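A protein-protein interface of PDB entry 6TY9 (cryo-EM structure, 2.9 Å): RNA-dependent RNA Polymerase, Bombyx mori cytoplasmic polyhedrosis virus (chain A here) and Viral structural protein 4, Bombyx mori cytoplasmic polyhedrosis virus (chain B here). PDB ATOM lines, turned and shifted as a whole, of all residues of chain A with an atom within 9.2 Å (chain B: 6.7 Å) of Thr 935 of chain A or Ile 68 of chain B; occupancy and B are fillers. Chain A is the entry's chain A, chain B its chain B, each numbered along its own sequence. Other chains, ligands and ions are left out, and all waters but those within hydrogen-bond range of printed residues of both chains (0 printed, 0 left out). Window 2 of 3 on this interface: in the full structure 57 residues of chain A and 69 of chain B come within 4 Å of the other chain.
Printed residues of chain A that touch a printed residue of chain B: Ala 457, Thr 935, Ser 936, Gln 939 and Leu 943.
Hydrophobic or aromatic side chains of chain A that line the printed part of chain B: Leu 943.
Of the 12 printed residues of chain B, 6 touch a printed residue of chain A.
Printed residues of chain B that touch a printed residue of chain A: Thr 66, Leu 67, Ile 68, Asn 69, Pro 70 and Arg 71.
Along chain B the printed residues that touch a printed residue of chain A span positions 66 to 71.
Among the printed residues, no Asp or Glu carboxylate lies within 4 Å of a Lys or Arg side-chain nitrogen of the other chain.
N of Leu 67 of chain B lies within hydrogen-bond range of OE1 of Gln 174 of chain B (3.2 Å).
The backbone carbonyl oxygen of Asn 931 of chain A sits at hydrogen-bond distance from the side-chain hydroxyl of Thr 935 of chain A.
The backbone carbonyl oxygen of His 63 of chain B is in hydrogen-bond range of the side-chain hydroxyl of Thr 66 of chain B (3.0 Å).
The backbone carbonyl oxygen (O) of Thr 935 of chain A sits close to the side-chain amide oxygen (OE1) of Gln 939 of chain A (2.9 Å).
The side-chain amide oxygen (OE1) of Gln 939 of chain A lies close to the backbone carbonyl oxygen (O) of Ile 68 of chain B, at 3.4 Å.
The guanidinium group (NH1) of Arg 71 of chain B is in hydrogen-bond range of the backbone carbonyl oxygen (O) of Leu 943 of chain A.
Among the printed residues, merely in contact across the chains: Ala 457 of chain A with Thr 66 of chain B (3.98 Å), Thr 935 of chain A with Ile 68 of chain B (3.8 Å), Ser 936 of chain A with Thr 66 of chain B (3.6 Å), Gln 939 of chain A with Leu 67 of chain B (3.7 Å), Gln 939 of chain A with Asn 69 of chain B (3.996 Å), Gln 939 of chain A with Pro 70 of chain B (3.6 Å), Leu 943 of chain A with Asn 69 of chain B (3.3 Å) and Leu 943 of chain A with Pro 70 of chain B (3.9 Å).
Thr 935 of chain A touches just one residue of chain B: Ile 68.
Ile 68 of chain B touches just these residues of chain A: Thr 935 (3.8 Å) and Gln 939 (2.2 Å).
Of the printed residues of chain A, Leu 67 of chain B touches Gln 939 (3.7 Å).
Of the printed residues of chain B, Leu 943 of chain A touches Asn 69 (3.3 Å), Pro 70 (3.9 Å) and Arg 71 (3.4 Å).
Of the printed residues of chain B, Gln 939 of chain A touches Leu 67 (3.7 Å), Ile 68 (2.2 Å), Asn 69 (3.996 Å) and Pro 70 (3.6 Å).
Gly 941 of chain A touches none of the printed residues of chain B.
Gln 174 of chain B touches none of the printed residues of chain A.
The nearest residue of chain B that does not touch Thr 935 of chain A is His 63 of chain B (5.9 Å).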
ATOM      1  N   LEU A 418      20.872 -15.262  -4.673  1.00  0.00           N
ATOM      2  CA  LEU A 418      20.513 -14.591  -3.429  1.00  0.00           C
ATOM      3  C   LEU A 418      20.233 -13.116  -3.661  1.00  0.00           C
ATOM      4  O   LEU A 418      19.413 -12.515  -2.960  1.00  0.00           O
ATOM      5  CB  LEU A 418      21.622 -14.766  -2.398  1.00  0.00           C
ATOM      6  CG  LEU A 418      21.712 -16.142  -1.752  1.00  0.00           C
ATOM      7  CD1 LEU A 418      22.656 -16.097  -0.583  1.00  0.00           C
ATOM      8  CD2 LEU A 418      20.342 -16.597  -1.310  1.00  0.00           C
ATOM      9  N   ALA A 454      15.224 -18.302   3.696  1.00  0.00           N
ATOM     10  CA  ALA A 454      15.977 -18.428   4.936  1.00  0.00           C
ATOM     11  C   ALA A 454      15.425 -19.533   5.818  1.00  0.00           C
ATOM     12  O   ALA A 454      16.193 -20.229   6.488  1.00  0.00           O
ATOM     13  CB  ALA A 454      15.969 -17.106   5.693  1.00  0.00           C
ATOM     14  N   ALA A 457      16.476 -22.926   4.288  1.00  0.00           N
ATOM     15  CA  ALA A 457      17.872 -22.944   3.887  1.00  0.00           C
ATOM     16  C   ALA A 457      18.536 -24.291   4.108  1.00  0.00           C
ATOM     17  O   ALA A 457      19.579 -24.548   3.505  1.00  0.00           O
ATOM     18  CB  ALA A 457      18.642 -21.863   4.640  1.00  0.00           C
ATOM     19  N   PRO A 927      15.650  -8.451  16.889  1.00  0.00           N
ATOM     20  CA  PRO A 927      16.879  -8.615  16.101  1.00  0.00           C
ATOM     21  C   PRO A 927      17.544  -9.964  16.294  1.00  0.00           C
ATOM     22  O   PRO A 927      18.425 -10.319  15.504  1.00  0.00           O
ATOM     23  CB  PRO A 927      17.775  -7.474  16.602  1.00  0.00           C
ATOM     24  CG  PRO A 927      16.855  -6.535  17.309  1.00  0.00           C
ATOM     25  CD  PRO A 927      15.789  -7.391  17.895  1.00  0.00           C
ATOM     26  N   VAL A 928      17.167 -10.720  17.325  1.00  0.00           N
ATOM     27  CA  VAL A 928      17.704 -12.067  17.493  1.00  0.00           C
ATOM     28  C   VAL A 928      17.194 -12.975  16.382  1.00  0.00           C
ATOM     29  O   VAL A 928      17.922 -13.836  15.875  1.00  0.00           O
ATOM     30  CB  VAL A 928      17.355 -12.613  18.889  1.00  0.00           C
ATOM     31  CG1 VAL A 928      17.417 -14.130  18.910  1.00  0.00           C
ATOM     32  CG2 VAL A 928      18.299 -12.036  19.921  1.00  0.00           C
ATOM     33  N   LYS A 929      15.940 -12.783  15.973  1.00  0.00           N
ATOM     34  CA  LYS A 929      15.395 -13.592  14.890  1.00  0.00           C
ATOM     35  C   LYS A 929      15.900 -13.130  13.532  1.00  0.00           C
ATOM     36  O   LYS A 929      16.152 -13.961  12.656  1.00  0.00           O
ATOM     37  CB  LYS A 929      13.871 -13.559  14.929  1.00  0.00           C
ATOM     38  CG  LYS A 929      13.264 -14.575  15.874  1.00  0.00           C
ATOM     39  CD  LYS A 929      13.914 -15.939  15.712  1.00  0.00           C
ATOM     40  CE  LYS A 929      13.035 -17.033  16.287  1.00  0.00           C
ATOM     41  NZ  LYS A 929      12.348 -16.584  17.530  1.00  0.00           N
ATOM     42  N   VAL A 930      16.049 -11.822  13.334  1.00  0.00           N
ATOM     43  CA  VAL A 930      16.566 -11.321  12.066  1.00  0.00           C
ATOM     44  C   VAL A 930      18.004 -11.774  11.864  1.00  0.00           C
ATOM     45  O   VAL A 930      18.419 -12.093  10.744  1.00  0.00           O
ATOM     46  CB  VAL A 930      16.443  -9.787  12.006  1.00  0.00           C
ATOM     47  CG1 VAL A 930      17.089  -9.248  10.741  1.00  0.00           C
ATOM     48  CG2 VAL A 930      14.989  -9.372  12.080  1.00  0.00           C
ATOM     49  N   ASN A 931      18.787 -11.821  12.941  1.00  0.00           N
ATOM     50  CA  ASN A 931      20.183 -12.220  12.809  1.00  0.00           C
ATOM     51  C   ASN A 931      20.303 -13.722  12.591  1.00  0.00           C
ATOM     52  O   ASN A 931      21.103 -14.170  11.763  1.00  0.00           O
ATOM     53  CB  ASN A 931      20.975 -11.786  14.039  1.00  0.00           C
ATOM     54  CG  ASN A 931      22.476 -11.854  13.818  1.00  0.00           C
ATOM     55  OD1 ASN A 931      22.942 -12.225  12.742  1.00  0.00           O
ATOM     56  ND2 ASN A 931      23.242 -11.494  14.842  1.00  0.00           N
ATOM     57  N   GLU A 932      19.513 -14.516  13.316  1.00  0.00           N
ATOM     58  CA  GLU A 932      19.504 -15.956  13.081  1.00  0.00           C
ATOM     59  C   GLU A 932      19.053 -16.281  11.665  1.00  0.00           C
ATOM     60  O   GLU A 932      19.590 -17.194  11.032  1.00  0.00           O
ATOM     61  CB  GLU A 932      18.594 -16.654  14.086  1.00  0.00           C
ATOM     62  CG  GLU A 932      19.242 -16.963  15.414  1.00  0.00           C
ATOM     63  CD  GLU A 932      18.234 -17.427  16.438  1.00  0.00           C
ATOM     64  OE1 GLU A 932      17.324 -18.195  16.061  1.00  0.00           O
ATOM     65  OE2 GLU A 932      18.345 -17.023  17.615  1.00  0.00           O
ATOM     66  N   LEU A 933      18.059 -15.554  11.156  1.00  0.00           N
ATOM     67  CA  LEU A 933      17.606 -15.788   9.792  1.00  0.00           C
ATOM     68  C   LEU A 933      18.661 -15.362   8.784  1.00  0.00           C
ATOM     69  O   LEU A 933      18.836 -16.013   7.749  1.00  0.00           O
ATOM     70  CB  LEU A 933      16.299 -15.043   9.537  1.00  0.00           C
ATOM     71  CG  LEU A 933      15.007 -15.723   9.981  1.00  0.00           C
ATOM     72  CD1 LEU A 933      13.815 -14.914   9.517  1.00  0.00           C
ATOM     73  CD2 LEU A 933      14.929 -17.142   9.458  1.00  0.00           C
ATOM     74  N   ALA A 934      19.367 -14.270   9.064  1.00  0.00           N
ATOM     75  CA  ALA A 934      20.405 -13.809   8.152  1.00  0.00           C
ATOM     76  C   ALA A 934      21.617 -14.726   8.190  1.00  0.00           C
ATOM     77  O   ALA A 934      22.314 -14.881   7.183  1.00  0.00           O
ATOM     78  CB  ALA A 934      20.807 -12.377   8.494  1.00  0.00           C
ATOM     79  N   THR A 935      21.886 -15.339   9.342  1.00  0.00           N
ATOM     80  CA  THR A 935      23.023 -16.244   9.442  1.00  0.00           C
ATOM     81  C   THR A 935      22.850 -17.448   8.528  1.00  0.00           C
ATOM     82  O   THR A 935      23.809 -17.891   7.890  1.00  0.00           O
ATOM     83  CB  THR A 935      23.210 -16.689  10.891  1.00  0.00           C
ATOM     84  OG1 THR A 935      23.589 -15.562  11.687  1.00  0.00           O
ATOM     85  CG2 THR A 935      24.290 -17.744  10.995  1.00  0.00           C
ATOM     86  N   SER A 936      21.633 -17.980   8.435  1.00  0.00           N
ATOM     87  CA  SER A 936      21.395 -19.165   7.626  1.00  0.00           C
ATOM     88  C   SER A 936      21.369 -18.862   6.134  1.00  0.00           C
ATOM     89  O   SER A 936      21.599 -19.769   5.331  1.00  0.00           O
ATOM     90  CB  SER A 936      20.090 -19.826   8.047  1.00  0.00           C
ATOM     91  OG  SER A 936      20.250 -20.503   9.278  1.00  0.00           O
ATOM     92  N   LEU A 937      21.091 -17.622   5.744  1.00  0.00           N
ATOM     93  CA  LEU A 937      21.169 -17.269   4.333  1.00  0.00           C
ATOM     94  C   LEU A 937      22.603 -17.067   3.871  1.00  0.00           C
ATOM     95  O   LEU A 937      22.879 -17.165   2.672  1.00  0.00           O
ATOM     96  CB  LEU A 937      20.360 -16.007   4.050  1.00  0.00           C
ATOM     97  CG  LEU A 937      18.904 -16.200   3.656  1.00  0.00           C
ATOM     98  CD1 LEU A 937      18.219 -14.861   3.553  1.00  0.00           C
ATOM     99  CD2 LEU A 937      18.829 -16.939   2.340  1.00  0.00           C
ATOM    100  N   GLU A 938      23.519 -16.777   4.792  1.00  0.00           N
ATOM    101  CA  GLU A 938      24.910 -16.571   4.421  1.00  0.00           C
ATOM    102  C   GLU A 938      25.630 -17.868   4.097  1.00  0.00           C
ATOM    103  O   GLU A 938      26.679 -17.824   3.448  1.00  0.00           O
ATOM    104  CB  GLU A 938      25.647 -15.837   5.538  1.00  0.00           C
ATOM    105  CG  GLU A 938      25.211 -14.399   5.702  1.00  0.00           C
ATOM    106  CD  GLU A 938      25.606 -13.822   7.043  1.00  0.00           C
ATOM    107  OE1 GLU A 938      26.337 -14.502   7.790  1.00  0.00           O
ATOM    108  OE2 GLU A 938      25.178 -12.691   7.352  1.00  0.00           O
ATOM    109  N   GLN A 939      25.096 -19.010   4.520  1.00  0.00           N
ATOM    110  CA  GLN A 939      25.682 -20.309   4.226  1.00  0.00           C
ATOM    111  C   GLN A 939      25.278 -20.828   2.857  1.00  0.00           C
ATOM    112  O   GLN A 939      25.455 -22.016   2.577  1.00  0.00           O
ATOM    113  CB  GLN A 939      25.284 -21.322   5.295  1.00  0.00           C
ATOM    114  CG  GLN A 939      25.325 -20.804   6.712  1.00  0.00           C
ATOM    115  CD  GLN A 939      26.566 -20.010   7.010  1.00  0.00           C
ATOM    116  OE1 GLN A 939      26.494 -18.897   7.519  1.00  0.00           O
ATOM    117  NE2 GLN A 939      27.717 -20.573   6.693  1.00  0.00           N
ATOM    118  N   LEU A 940      24.738 -19.968   2.008  1.00  0.00           N
ATOM    119  CA  LEU A 940      24.229 -20.359   0.706  1.00  0.00           C
ATOM    120  C   LEU A 940      24.973 -19.717  -0.447  1.00  0.00           C
ATOM    121  O   LEU A 940      24.940 -20.250  -1.555  1.00  0.00           O
ATOM    122  CB  LEU A 940      22.738 -20.008   0.594  1.00  0.00           C
ATOM    123  CG  LEU A 940      21.705 -21.086   0.931  1.00  0.00           C
ATOM    124  CD1 LEU A 940      21.864 -21.597   2.342  1.00  0.00           C
ATOM    125  CD2 LEU A 940      20.310 -20.550   0.731  1.00  0.00           C
ATOM    126  N   GLY A 941      25.641 -18.592  -0.223  1.00  0.00           N
ATOM    127  CA  GLY A 941      26.393 -17.956  -1.279  1.00  0.00           C
ATOM    128  C   GLY A 941      27.714 -17.374  -0.832  1.00  0.00           C
ATOM    129  O   GLY A 941      27.771 -16.562   0.094  1.00  0.00           O
ATOM    130  N   LEU A 943      30.168 -17.788   0.950  1.00  0.00           N
ATOM    131  CA  LEU A 943      30.824 -18.062   2.230  1.00  0.00           C
ATOM    132  C   LEU A 943      31.712 -16.896   2.665  1.00  0.00           C
ATOM    133  O   LEU A 943      32.936 -16.997   2.744  1.00  0.00           O
ATOM    134  CB  LEU A 943      31.609 -19.371   2.157  1.00  0.00           C
ATOM    135  CG  LEU A 943      30.905 -20.596   2.735  1.00  0.00           C
ATOM    136  CD1 LEU A 943      31.026 -20.577   4.232  1.00  0.00           C
ATOM    137  CD2 LEU A 943      29.442 -20.548   2.377  1.00  0.00           C
ATOM    138  N   GLY A 944      31.064 -15.772   2.927  1.00  0.00           N
ATOM    139  CA  GLY A 944      31.760 -14.560   3.299  1.00  0.00           C
ATOM    140  C   GLY A 944      31.185 -13.366   2.570  1.00  0.00           C
ATOM    141  O   GLY A 944      30.016 -13.384   2.181  1.00  0.00           O
ATOM    142  N   ARG A 946      29.752 -10.908   3.159  1.00  0.00           N
ATOM    143  CA  ARG A 946      28.792 -10.133   3.928  1.00  0.00           C
ATOM    144  C   ARG A 946      29.432  -9.530   5.161  1.00  0.00           C
ATOM    145  O   ARG A 946      29.284  -8.334   5.410  1.00  0.00           O
ATOM    146  CB  ARG A 946      27.609 -11.004   4.361  1.00  0.00           C
ATOM    147  CG  ARG A 946      26.875 -11.700   3.241  1.00  0.00           C
ATOM    148  CD  ARG A 946      26.531 -10.747   2.135  1.00  0.00           C
ATOM    149  NE  ARG A 946      25.597 -11.333   1.182  1.00  0.00           N
ATOM    150  CZ  ARG A 946      24.371 -10.877   0.966  1.00  0.00           C
ATOM    151  NH1 ARG A 946      23.933  -9.818   1.628  1.00  0.00           N
ATOM    152  NH2 ARG A 946      23.587 -11.470   0.077  1.00  0.00           N
ATOM    153  N   ARG A 950      30.308  -5.657   5.621  1.00  0.00           N
ATOM    154  CA  ARG A 950      29.778  -5.042   6.832  1.00  0.00           C
ATOM    155  C   ARG A 950      30.881  -4.395   7.652  1.00  0.00           C
ATOM    156  O   ARG A 950      30.704  -3.287   8.164  1.00  0.00           O
ATOM    157  CB  ARG A 950      29.040  -6.079   7.676  1.00  0.00           C
ATOM    158  CG  ARG A 950      27.535  -6.054   7.512  1.00  0.00           C
ATOM    159  CD  ARG A 950      26.853  -7.051   8.436  1.00  0.00           C
ATOM    160  NE  ARG A 950      26.823  -8.396   7.873  1.00  0.00           N
ATOM    161  CZ  ARG A 950      27.533  -9.413   8.344  1.00  0.00           C
ATOM    162  NH1 ARG A 950      27.447 -10.604   7.773  1.00  0.00           N
ATOM    163  NH2 ARG A 950      28.329  -9.240   9.387  1.00  0.00           N
ATOM    164  N   GLY A 970      26.411  -5.671   3.094  1.00  0.00           N
ATOM    165  CA  GLY A 970      26.344  -6.633   4.178  1.00  0.00           C
ATOM    166  C   GLY A 970      25.033  -6.643   4.933  1.00  0.00           C
ATOM    167  O   GLY A 970      24.679  -7.679   5.505  1.00  0.00           O
ATOM    168  N   LEU A 973      20.658  -8.443   3.462  1.00  0.00           N
ATOM    169  CA  LEU A 973      19.739  -9.480   3.918  1.00  0.00           C
ATOM    170  C   LEU A 973      18.815  -8.961   5.011  1.00  0.00           C
ATOM    171  O   LEU A 973      17.629  -9.306   5.040  1.00  0.00           O
ATOM    172  CB  LEU A 973      20.525 -10.691   4.409  1.00  0.00           C
ATOM    173  CG  LEU A 973      21.429 -11.365   3.375  1.00  0.00           C
ATOM    174  CD1 LEU A 973      21.755 -12.771   3.806  1.00  0.00           C
ATOM    175  CD2 LEU A 973      20.781 -11.377   2.003  1.00  0.00           C
ATOM    176  N   GLN A 974      19.335  -8.132   5.919  1.00  0.00           N
ATOM    177  CA  GLN A 974      18.513  -7.647   7.022  1.00  0.00           C
ATOM    178  C   GLN A 974      17.456  -6.662   6.541  1.00  0.00           C
ATOM    179  O   GLN A 974      16.282  -6.777   6.908  1.00  0.00           O
ATOM    180  CB  GLN A 974      19.383  -7.003   8.100  1.00  0.00           C
ATOM    181  CG  GLN A 974      20.157  -7.982   8.959  1.00  0.00           C
ATOM    182  CD  GLN A 974      21.527  -8.292   8.405  1.00  0.00           C
ATOM    183  OE1 GLN A 974      21.823  -9.428   8.051  1.00  0.00           O
ATOM    184  NE2 GLN A 974      22.383  -7.284   8.352  1.00  0.00           N
ATOM    185  N   ILE A 977      14.383  -8.303   5.509  1.00  0.00           N
ATOM    186  CA  ILE A 977      13.646  -8.947   6.592  1.00  0.00           C
ATOM    187  C   ILE A 977      13.016  -7.901   7.504  1.00  0.00           C
ATOM    188  O   ILE A 977      11.998  -8.160   8.156  1.00  0.00           O
ATOM    189  CB  ILE A 977      14.567  -9.910   7.366  1.00  0.00           C
ATOM    190  CG1 ILE A 977      15.260 -10.864   6.397  1.00  0.00           C
ATOM    191  CG2 ILE A 977      13.774 -10.724   8.360  1.00  0.00           C
ATOM    192  CD1 ILE A 977      16.287 -11.761   7.049  1.00  0.00           C
ATOM    193  N   HIS B  59      25.365 -31.285  15.249  1.00  0.00           N
ATOM    194  CA  HIS B  59      25.698 -29.884  15.023  1.00  0.00           C
ATOM    195  C   HIS B  59      24.672 -29.198  14.141  1.00  0.00           C
ATOM    196  O   HIS B  59      24.367 -28.020  14.349  1.00  0.00           O
ATOM    197  CB  HIS B  59      27.080 -29.757  14.383  1.00  0.00           C
ATOM    198  CG  HIS B  59      28.212 -30.027  15.319  1.00  0.00           C
ATOM    199  ND1 HIS B  59      28.358 -29.367  16.517  1.00  0.00           N
ATOM    200  CD2 HIS B  59      29.268 -30.864  15.222  1.00  0.00           C
ATOM    201  CE1 HIS B  59      29.444 -29.801  17.129  1.00  0.00           C
ATOM    202  NE2 HIS B  59      30.016 -30.709  16.362  1.00  0.00           N
ATOM    203  N   HIS B  63      21.446 -25.172  14.609  1.00  0.00           N
ATOM    204  CA  HIS B  63      21.153 -23.938  13.884  1.00  0.00           C
ATOM    205  C   HIS B  63      20.227 -24.274  12.724  1.00  0.00           C
ATOM    206  O   HIS B  63      20.669 -24.406  11.583  1.00  0.00           O
ATOM    207  CB  HIS B  63      22.436 -23.271  13.406  1.00  0.00           C
ATOM    208  CG  HIS B  63      23.384 -22.924  14.511  1.00  0.00           C
ATOM    209  ND1 HIS B  63      24.280 -23.830  15.035  1.00  0.00           N
ATOM    210  CD2 HIS B  63      23.575 -21.770  15.192  1.00  0.00           C
ATOM    211  CE1 HIS B  63      24.981 -23.248  15.991  1.00  0.00           C
ATOM    212  NE2 HIS B  63      24.573 -21.998  16.106  1.00  0.00           N
ATOM    213  N   THR B  66      21.251 -26.302   9.601  1.00  0.00           N
ATOM    214  CA  THR B  66      22.371 -25.966   8.736  1.00  0.00           C
ATOM    215  C   THR B  66      23.681 -25.975   9.510  1.00  0.00           C
ATOM    216  O   THR B  66      23.732 -25.650  10.698  1.00  0.00           O
ATOM    217  CB  THR B  66      22.185 -24.588   8.097  1.00  0.00           C
ATOM    218  OG1 THR B  66      22.098 -23.598   9.125  1.00  0.00           O
ATOM    219  CG2 THR B  66      20.932 -24.547   7.273  1.00  0.00           C
ATOM    220  N   LEU B  67      24.752 -26.339   8.815  1.00  0.00           N
ATOM    221  CA  LEU B  67      26.104 -26.169   9.324  1.00  0.00           C
ATOM    222  C   LEU B  67      26.562 -24.745   9.044  1.00  0.00           C
ATOM    223  O   LEU B  67      26.265 -24.182   7.990  1.00  0.00           O
ATOM    224  CB  LEU B  67      27.065 -27.172   8.686  1.00  0.00           C
ATOM    225  CG  LEU B  67      26.711 -28.649   8.855  1.00  0.00           C
ATOM    226  CD1 LEU B  67      27.390 -29.488   7.800  1.00  0.00           C
ATOM    227  CD2 LEU B  67      27.093 -29.125  10.231  1.00  0.00           C
ATOM    228  N   ILE B  68      27.281 -24.164   9.999  1.00  0.00           N
ATOM    229  CA  ILE B  68      27.540 -22.729   9.986  1.00  0.00           C
ATOM    230  C   ILE B  68      28.706 -22.381   9.069  1.00  0.00           C
ATOM    231  O   ILE B  68      28.756 -21.284   8.505  1.00  0.00           O
ATOM    232  CB  ILE B  68      27.766 -22.207  11.416  1.00  0.00           C
ATOM    233  CG1 ILE B  68      26.428 -22.126  12.142  1.00  0.00           C
ATOM    234  CG2 ILE B  68      28.428 -20.847  11.416  1.00  0.00           C
ATOM    235  CD1 ILE B  68      25.378 -21.367  11.376  1.00  0.00           C
ATOM    236  N   ASN B  69      29.640 -23.308   8.881  1.00  0.00           N
ATOM    237  CA  ASN B  69      30.743 -23.089   7.947  1.00  0.00           C
ATOM    238  C   ASN B  69      30.951 -24.359   7.148  1.00  0.00           C
ATOM    239  O   ASN B  69      31.845 -25.159   7.444  1.00  0.00           O
ATOM    240  CB  ASN B  69      32.025 -22.686   8.672  1.00  0.00           C
ATOM    241  CG  ASN B  69      33.016 -21.997   7.762  1.00  0.00           C
ATOM    242  OD1 ASN B  69      32.899 -22.055   6.542  1.00  0.00           O
ATOM    243  ND2 ASN B  69      34.006 -21.350   8.353  1.00  0.00           N
ATOM    244  N   PRO B  70      30.141 -24.579   6.112  1.00  0.00           N
ATOM    245  CA  PRO B  70      30.239 -25.840   5.366  1.00  0.00           C
ATOM    246  C   PRO B  70      31.575 -26.043   4.672  1.00  0.00           C
ATOM    247  O   PRO B  70      31.847 -27.159   4.221  1.00  0.00           O
ATOM    248  CB  PRO B  70      29.094 -25.735   4.352  1.00  0.00           C
ATOM    249  CG  PRO B  70      28.835 -24.286   4.225  1.00  0.00           C
ATOM    250  CD  PRO B  70      29.096 -23.699   5.568  1.00  0.00           C
ATOM    251  N   ARG B  71      32.415 -25.014   4.569  1.00  0.00           N
ATOM    252  CA  ARG B  71      33.709 -25.190   3.921  1.00  0.00           C
ATOM    253  C   ARG B  71      34.770 -25.654   4.907  1.00  0.00           C
ATOM    254  O   ARG B  71      35.627 -26.469   4.553  1.00  0.00           O
ATOM    255  CB  ARG B  71      34.146 -23.895   3.247  1.00  0.00           C
ATOM    256  CG  ARG B  71      35.416 -24.032   2.442  1.00  0.00           C
ATOM    257  CD  ARG B  71      35.602 -22.862   1.504  1.00  0.00           C
ATOM    258  NE  ARG B  71      35.687 -21.599   2.227  1.00  0.00           N
ATOM    259  CZ  ARG B  71      35.325 -20.426   1.723  1.00  0.00           C
ATOM    260  NH1 ARG B  71      35.436 -19.326   2.454  1.00  0.00           N
ATOM    261  NH2 ARG B  71      34.853 -20.351   0.488  1.00  0.00           N
ATOM    262  N   TYR B  73      34.061 -27.445   7.553  1.00  0.00           N
ATOM    263  CA  TYR B  73      33.682 -28.828   7.816  1.00  0.00           C
ATOM    264  C   TYR B  73      34.189 -29.753   6.726  1.00  0.00           C
ATOM    265  O   TYR B  73      34.721 -30.829   7.011  1.00  0.00           O
ATOM    266  CB  TYR B  73      32.165 -28.948   7.922  1.00  0.00           C
ATOM    267  CG  TYR B  73      31.603 -28.575   9.263  1.00  0.00           C
ATOM    268  CD1 TYR B  73      31.691 -29.443  10.332  1.00  0.00           C
ATOM    269  CD2 TYR B  73      30.969 -27.362   9.454  1.00  0.00           C
ATOM    270  CE1 TYR B  73      31.174 -29.110  11.553  1.00  0.00           C
ATOM    271  CE2 TYR B  73      30.453 -27.022  10.672  1.00  0.00           C
ATOM    272  CZ  TYR B  73      30.556 -27.900  11.717  1.00  0.00           C
ATOM    273  OH  TYR B  73      30.038 -27.564  12.937  1.00  0.00           O
ATOM    274  N   THR B 134      31.696 -18.963  18.617  1.00  0.00           N
ATOM    275  CA  THR B 134      31.429 -19.175  17.201  1.00  0.00           C
ATOM    276  C   THR B 134      32.170 -20.389  16.662  1.00  0.00           C
ATOM    277  O   THR B 134      31.670 -21.060  15.753  1.00  0.00           O
ATOM    278  CB  THR B 134      31.802 -17.930  16.394  1.00  0.00           C
ATOM    279  OG1 THR B 134      33.219 -17.893  16.189  1.00  0.00           O
ATOM    280  CG2 THR B 134      31.376 -16.677  17.136  1.00  0.00           C
ATOM    281  N   LEU B 138      33.292 -26.170  15.658  1.00  0.00           N
ATOM    282  CA  LEU B 138      34.446 -26.555  14.855  1.00  0.00           C
ATOM    283  C   LEU B 138      35.600 -27.027  15.722  1.00  0.00           C
ATOM    284  O   LEU B 138      36.389 -27.870  15.287  1.00  0.00           O
ATOM    285  CB  LEU B 138      34.882 -25.389  13.975  1.00  0.00           C
ATOM    286  CG  LEU B 138      34.076 -25.243  12.689  1.00  0.00           C
ATOM    287  CD1 LEU B 138      34.461 -23.970  11.973  1.00  0.00           C
ATOM    288  CD2 LEU B 138      34.293 -26.444  11.800  1.00  0.00           C
ATOM    289  N   GLN B 174      25.044 -30.330   2.052  1.00  0.00           N
ATOM    290  CA  GLN B 174      25.676 -29.024   2.178  1.00  0.00           C
ATOM    291  C   GLN B 174      27.188 -29.120   2.054  1.00  0.00           C
ATOM    292  O   GLN B 174      27.845 -28.127   1.729  1.00  0.00           O
ATOM    293  CB  GLN B 174      25.287 -28.383   3.506  1.00  0.00           C
ATOM    294  CG  GLN B 174      23.801 -28.400   3.759  1.00  0.00           C
ATOM    295  CD  GLN B 174      23.443 -28.055   5.180  1.00  0.00           C
ATOM    296  OE1 GLN B 174      24.233 -27.454   5.900  1.00  0.00           O
ATOM    297  NE2 GLN B 174      22.243 -28.431   5.592  1.00  0.00           N
